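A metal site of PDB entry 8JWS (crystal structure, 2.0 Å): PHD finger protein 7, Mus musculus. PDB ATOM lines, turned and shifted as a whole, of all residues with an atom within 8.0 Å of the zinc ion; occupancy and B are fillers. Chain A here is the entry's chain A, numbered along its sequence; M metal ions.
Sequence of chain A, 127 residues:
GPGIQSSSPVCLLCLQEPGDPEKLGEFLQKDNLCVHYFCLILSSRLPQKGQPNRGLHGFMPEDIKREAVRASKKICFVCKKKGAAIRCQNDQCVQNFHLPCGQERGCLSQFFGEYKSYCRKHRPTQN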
ATOM      1  N   CYS A  14      23.520 -34.949   1.074  1.00  0.00           N
ATOM      2  CA  CYS A  14      22.198 -34.355   1.147  1.00  0.00           C
ATOM      3  C   CYS A  14      21.341 -34.895   2.293  1.00  0.00           C
ATOM      4  O   CYS A  14      20.299 -34.332   2.587  1.00  0.00           O
ATOM      5  CB  CYS A  14      21.460 -34.482  -0.191  1.00  0.00           C
ATOM      6  SG  CYS A  14      20.867 -36.139  -0.561  1.00  0.00           S
ATOM      7  N   LEU A  15      21.776 -35.994   2.904  1.00  0.00           N
ATOM      8  CA  LEU A  15      21.124 -36.639   4.043  1.00  0.00           C
ATOM      9  C   LEU A  15      19.785 -37.293   3.699  1.00  0.00           C
ATOM     10  O   LEU A  15      19.023 -37.620   4.603  1.00  0.00           O
ATOM     11  CB  LEU A  15      20.966 -35.617   5.187  1.00  0.00           C
ATOM     12  CG  LEU A  15      22.235 -34.880   5.582  1.00  0.00           C
ATOM     13  CD1 LEU A  15      21.922 -33.809   6.644  1.00  0.00           C
ATOM     14  CD2 LEU A  15      23.269 -35.839   6.110  1.00  0.00           C
ATOM     15  N   GLN A  16      19.513 -37.483   2.398  1.00  0.00           N
ATOM     16  CA  GLN A  16      18.277 -38.107   1.957  1.00  0.00           C
ATOM     17  C   GLN A  16      18.476 -39.526   1.415  1.00  0.00           C
ATOM     18  O   GLN A  16      19.586 -39.943   1.114  1.00  0.00           O
ATOM     19  CB  GLN A  16      17.603 -37.269   0.868  1.00  0.00           C
ATOM     20  CG  GLN A  16      17.097 -35.915   1.432  1.00  0.00           C
ATOM     21  CD  GLN A  16      16.128 -35.235   0.506  1.00  0.00           C
ATOM     22  OE1 GLN A  16      15.500 -35.903  -0.348  1.00  0.00           O
ATOM     23  NE2 GLN A  16      15.981 -33.936   0.684  1.00  0.00           N
ATOM     24  N   LYS A  74      26.528 -25.277   7.025  1.00  0.00           N
ATOM     25  CA  LYS A  74      25.725 -24.483   6.098  1.00  0.00           C
ATOM     26  C   LYS A  74      24.258 -24.892   6.124  1.00  0.00           C
ATOM     27  O   LYS A  74      23.927 -26.072   6.059  1.00  0.00           O
ATOM     28  CB  LYS A  74      26.278 -24.574   4.675  1.00  0.00           C
ATOM     29  CG  LYS A  74      27.764 -24.161   4.548  1.00  0.00           C
ATOM     30  CD  LYS A  74      28.117 -22.775   4.968  1.00  0.00           C
ATOM     31  CE  LYS A  74      27.526 -21.763   4.041  1.00  0.00           C
ATOM     32  NZ  LYS A  74      28.004 -20.406   4.348  1.00  0.00           N
ATOM     33  N   ILE A  75      23.379 -23.892   6.236  1.00  0.00           N
ATOM     34  CA  ILE A  75      21.942 -24.099   6.286  1.00  0.00           C
ATOM     35  C   ILE A  75      21.354 -24.052   4.867  1.00  0.00           C
ATOM     36  O   ILE A  75      21.632 -23.143   4.086  1.00  0.00           O
ATOM     37  CB  ILE A  75      21.297 -23.064   7.241  1.00  0.00           C
ATOM     38  CG1 ILE A  75      21.835 -23.236   8.698  1.00  0.00           C
ATOM     39  CG2 ILE A  75      19.756 -23.127   7.201  1.00  0.00           C
ATOM     40  CD1 ILE A  75      21.402 -22.274   9.651  1.00  0.00           C
ATOM     41  N   CYS A  76      20.564 -25.073   4.546  1.00  0.00           N
ATOM     42  CA  CYS A  76      19.776 -25.115   3.312  1.00  0.00           C
ATOM     43  C   CYS A  76      18.623 -24.106   3.377  1.00  0.00           C
ATOM     44  O   CYS A  76      17.816 -24.137   4.310  1.00  0.00           O
ATOM     45  CB  CYS A  76      19.253 -26.529   3.124  1.00  0.00           C
ATOM     46  SG  CYS A  76      18.197 -26.790   1.660  1.00  0.00           S
ATOM     47  N   PHE A  77      18.536 -23.232   2.357  1.00  0.00           N
ATOM     48  CA  PHE A  77      17.511 -22.201   2.345  1.00  0.00           C
ATOM     49  C   PHE A  77      16.109 -22.803   2.194  1.00  0.00           C
ATOM     50  O   PHE A  77      15.134 -22.177   2.605  1.00  0.00           O
ATOM     51  CB  PHE A  77      17.779 -21.148   1.274  1.00  0.00           C
ATOM     52  CG  PHE A  77      17.358 -21.489  -0.138  1.00  0.00           C
ATOM     53  CD1 PHE A  77      16.066 -21.214  -0.578  1.00  0.00           C
ATOM     54  CD2 PHE A  77      18.256 -22.043  -1.031  1.00  0.00           C
ATOM     55  CE1 PHE A  77      15.688 -21.543  -1.886  1.00  0.00           C
ATOM     56  CE2 PHE A  77      17.864 -22.363  -2.333  1.00  0.00           C
ATOM     57  CZ  PHE A  77      16.594 -22.107  -2.744  1.00  0.00           C
ATOM     58  N   VAL A  78      16.026 -24.025   1.644  1.00  0.00           N
ATOM     59  CA  VAL A  78      14.733 -24.678   1.449  1.00  0.00           C
ATOM     60  C   VAL A  78      14.175 -25.306   2.725  1.00  0.00           C
ATOM     61  O   VAL A  78      13.073 -24.981   3.155  1.00  0.00           O
ATOM     62  CB  VAL A  78      14.820 -25.735   0.328  1.00  0.00           C
ATOM     63  CG1 VAL A  78      13.457 -26.362   0.062  1.00  0.00           C
ATOM     64  CG2 VAL A  78      15.407 -25.124  -0.937  1.00  0.00           C
ATOM     65  N   CYS A  79      14.930 -26.239   3.323  1.00  0.00           N
ATOM     66  CA  CYS A  79      14.436 -27.001   4.467  1.00  0.00           C
ATOM     67  C   CYS A  79      14.911 -26.444   5.816  1.00  0.00           C
ATOM     68  O   CYS A  79      14.454 -26.920   6.848  1.00  0.00           O
ATOM     69  CB  CYS A  79      14.791 -28.475   4.344  1.00  0.00           C
ATOM     70  SG  CYS A  79      16.569 -28.806   4.483  1.00  0.00           S
ATOM     71  N   LYS A  80      15.838 -25.476   5.790  1.00  0.00           N
ATOM     72  CA  LYS A  80      16.346 -24.803   6.984  1.00  0.00           C
ATOM     73  C   LYS A  80      17.166 -25.716   7.892  1.00  0.00           C
ATOM     74  O   LYS A  80      17.332 -25.442   9.066  1.00  0.00           O
ATOM     75  CB  LYS A  80      15.218 -24.196   7.818  1.00  0.00           C
ATOM     76  CG  LYS A  80      14.277 -23.236   7.091  1.00  0.00           C
ATOM     77  CD  LYS A  80      14.984 -22.134   6.419  1.00  0.00           C
ATOM     78  CE  LYS A  80      14.027 -21.001   6.040  1.00  0.00           C
ATOM     79  NZ  LYS A  80      14.431 -20.384   4.744  1.00  0.00           N
ATOM     80  N   LYS A  81      17.705 -26.807   7.333  1.00  0.00           N
ATOM     81  CA  LYS A  81      18.546 -27.725   8.086  1.00  0.00           C
ATOM     82  C   LYS A  81      19.977 -27.641   7.574  1.00  0.00           C
ATOM     83  O   LYS A  81      20.216 -27.211   6.449  1.00  0.00           O
ATOM     84  CB  LYS A  81      18.020 -29.160   7.960  1.00  0.00           C
ATOM     85  CG  LYS A  81      16.657 -29.370   8.538  1.00  0.00           C
ATOM     86  CD  LYS A  81      16.043 -30.655   8.048  1.00  0.00           C
ATOM     87  CE  LYS A  81      14.706 -30.864   8.669  1.00  0.00           C
ATOM     88  NZ  LYS A  81      14.052 -32.050   8.049  1.00  0.00           N
ATOM     89  N   LYS A  82      20.908 -28.092   8.420  1.00  0.00           N
ATOM     90  CA  LYS A  82      22.328 -28.082   8.105  1.00  0.00           C
ATOM     91  C   LYS A  82      22.661 -29.152   7.073  1.00  0.00           C
ATOM     92  O   LYS A  82      21.838 -29.995   6.747  1.00  0.00           O
ATOM     93  CB  LYS A  82      23.175 -28.337   9.381  1.00  0.00           C
ATOM     94  CG  LYS A  82      22.870 -27.469  10.565  1.00  0.00           C
ATOM     95  CD  LYS A  82      23.491 -26.133  10.454  1.00  0.00           C
ATOM     96  CE  LYS A  82      23.452 -25.416  11.783  1.00  0.00           C
ATOM     97  NZ  LYS A  82      24.317 -24.211  11.733  1.00  0.00           N
ATOM     98  N   GLY A  83      23.904 -29.113   6.578  1.00  0.00           N
ATOM     99  CA  GLY A  83      24.411 -30.099   5.633  1.00  0.00           C
ATOM    100  C   GLY A  83      24.308 -29.711   4.161  1.00  0.00           C
ATOM    101  O   GLY A  83      24.522 -30.552   3.297  1.00  0.00           O
ATOM    102  N   ALA A  84      24.020 -28.425   3.869  1.00  0.00           N
ATOM    103  CA  ALA A  84      23.881 -27.951   2.494  1.00  0.00           C
ATOM    104  C   ALA A  84      25.235 -27.840   1.800  1.00  0.00           C
ATOM    105  O   ALA A  84      26.046 -26.998   2.153  1.00  0.00           O
ATOM    106  CB  ALA A  84      23.166 -26.603   2.463  1.00  0.00           C
ATOM    107  N   ASN A  96      22.672 -21.512  -0.080  1.00  0.00           N
ATOM    108  CA  ASN A  96      23.177 -22.876  -0.114  1.00  0.00           C
ATOM    109  C   ASN A  96      21.990 -23.826  -0.011  1.00  0.00           C
ATOM    110  O   ASN A  96      20.961 -23.457   0.548  1.00  0.00           O
ATOM    111  CB  ASN A  96      24.147 -23.178   1.004  1.00  0.00           C
ATOM    112  CG  ASN A  96      25.380 -22.316   0.990  1.00  0.00           C
ATOM    113  OD1 ASN A  96      26.403 -22.736   0.480  1.00  0.00           O
ATOM    114  ND2 ASN A  96      25.308 -21.127   1.529  1.00  0.00           N
ATOM    115  N   PHE A  97      22.144 -25.039  -0.561  1.00  0.00           N
ATOM    116  CA  PHE A  97      21.052 -26.010  -0.527  1.00  0.00           C
ATOM    117  C   PHE A  97      21.530 -27.444  -0.695  1.00  0.00           C
ATOM    118  O   PHE A  97      22.610 -27.689  -1.217  1.00  0.00           O
ATOM    119  CB  PHE A  97      20.009 -25.664  -1.608  1.00  0.00           C
ATOM    120  CG  PHE A  97      20.539 -25.397  -2.990  1.00  0.00           C
ATOM    121  CD1 PHE A  97      21.004 -24.129  -3.341  1.00  0.00           C
ATOM    122  CD2 PHE A  97      20.584 -26.401  -3.941  1.00  0.00           C
ATOM    123  CE1 PHE A  97      21.466 -23.879  -4.633  1.00  0.00           C
ATOM    124  CE2 PHE A  97      21.064 -26.149  -5.225  1.00  0.00           C
ATOM    125  CZ  PHE A  97      21.491 -24.895  -5.561  1.00  0.00           C
ATOM    126  N   HIS A  98      20.712 -28.371  -0.179  1.00  0.00           N
ATOM    127  CA  HIS A  98      20.813 -29.782  -0.512  1.00  0.00           C
ATOM    128  C   HIS A  98      20.287 -29.951  -1.937  1.00  0.00           C
ATOM    129  O   HIS A  98      19.259 -29.356  -2.286  1.00  0.00           O
ATOM    130  CB  HIS A  98      19.990 -30.638   0.449  1.00  0.00           C
ATOM    131  CG  HIS A  98      20.270 -30.460   1.915  1.00  0.00           C
ATOM    132  ND1 HIS A  98      19.330 -29.959   2.788  1.00  0.00           N
ATOM    133  CD2 HIS A  98      21.351 -30.747   2.658  1.00  0.00           C
ATOM    134  CE1 HIS A  98      19.858 -29.927   4.023  1.00  0.00           C
ATOM    135  NE2 HIS A  98      21.080 -30.400   3.959  1.00  0.00           N
ATOM    136  N   LEU A  99      20.947 -30.777  -2.757  1.00  0.00           N
ATOM    137  CA  LEU A  99      20.504 -30.979  -4.140  1.00  0.00           C
ATOM    138  C   LEU A  99      19.015 -31.277  -4.289  1.00  0.00           C
ATOM    139  O   LEU A  99      18.328 -30.578  -5.034  1.00  0.00           O
ATOM    140  CB  LEU A  99      21.324 -32.095  -4.822  1.00  0.00           C
ATOM    141  CG  LEU A  99      20.986 -32.369  -6.262  1.00  0.00           C
ATOM    142  CD1 LEU A  99      21.145 -31.138  -7.076  1.00  0.00           C
ATOM    143  CD2 LEU A  99      21.862 -33.522  -6.838  1.00  0.00           C
ATOM    144  N   PRO A 100      18.443 -32.299  -3.591  1.00  0.00           N
ATOM    145  CA  PRO A 100      17.010 -32.603  -3.718  1.00  0.00           C
ATOM    146  C   PRO A 100      16.094 -31.429  -3.364  1.00  0.00           C
ATOM    147  O   PRO A 100      15.072 -31.219  -3.999  1.00  0.00           O
ATOM    148  CB  PRO A 100      16.806 -33.789  -2.779  1.00  0.00           C
ATOM    149  CG  PRO A 100      18.043 -33.835  -1.906  1.00  0.00           C
ATOM    150  CD  PRO A 100      19.138 -33.192  -2.647  1.00  0.00           C
ATOM    151  N   CYS A 101      16.501 -30.630  -2.366  1.00  0.00           N
ATOM    152  CA  CYS A 101      15.758 -29.464  -1.931  1.00  0.00           C
ATOM    153  C   CYS A 101      15.743 -28.373  -3.007  1.00  0.00           C
ATOM    154  O   CYS A 101      14.710 -27.769  -3.293  1.00  0.00           O
ATOM    155  CB  CYS A 101      16.343 -28.927  -0.636  1.00  0.00           C
ATOM    156  SG  CYS A 101      16.199 -30.027   0.797  1.00  0.00           S
ATOM    157  N   GLY A 102      16.921 -28.097  -3.571  1.00  0.00           N
ATOM    158  CA  GLY A 102      17.052 -27.145  -4.659  1.00  0.00           C
ATOM    159  C   GLY A 102      16.173 -27.506  -5.850  1.00  0.00           C
ATOM    160  O   GLY A 102      15.548 -26.633  -6.462  1.00  0.00           O
ATOM    161  N   GLU A 104      13.319 -28.841  -5.821  1.00  0.00           N
ATOM    162  CA  GLU A 104      11.924 -28.467  -5.531  1.00  0.00           C
ATOM    163  C   GLU A 104      11.677 -26.959  -5.675  1.00  0.00           C
ATOM    164  O   GLU A 104      10.534 -26.539  -5.712  1.00  0.00           O
ATOM    165  CB  GLU A 104      11.530 -28.884  -4.112  1.00  0.00           C
ATOM    166  CG  GLU A 104      11.728 -30.349  -3.780  1.00  0.00           C
ATOM    167  CD  GLU A 104      11.822 -30.608  -2.283  1.00  0.00           C
ATOM    168  OE1 GLU A 104      11.681 -29.660  -1.482  1.00  0.00           O
ATOM    169  OE2 GLU A 104      12.053 -31.770  -1.900  1.00  0.00           O
HETATM  170 ZN    ZN M   1      17.506 -28.925   2.373  1.00  0.00          ZN
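The backbone carbonyl oxygen (O) of Lys 82 sits at hydrogen-bond distance from a ring nitrogen (NE2) of His 98. The side-chain sulfur (SG) of Cys 79 sits close to the backbone NH (N) of Lys 81 (3.7 Å). The backbone NH (N) of Val 78 sits close to the side-chain sulfur (SG) of Cys 76, at 3.5 Å. N of Cys 76 is in hydrogen-bond range of O of Lys 81, at 2.9 Å.
ND1 of His 98 is bound to the zinc ion. SG of Cys 79 is bound to the zinc ion, at 2.3 Å. The zinc ion is bound by SG of Cys 101 (2.3 Å). The zinc ion is bound by SG of Cys 76 (2.4 Å).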
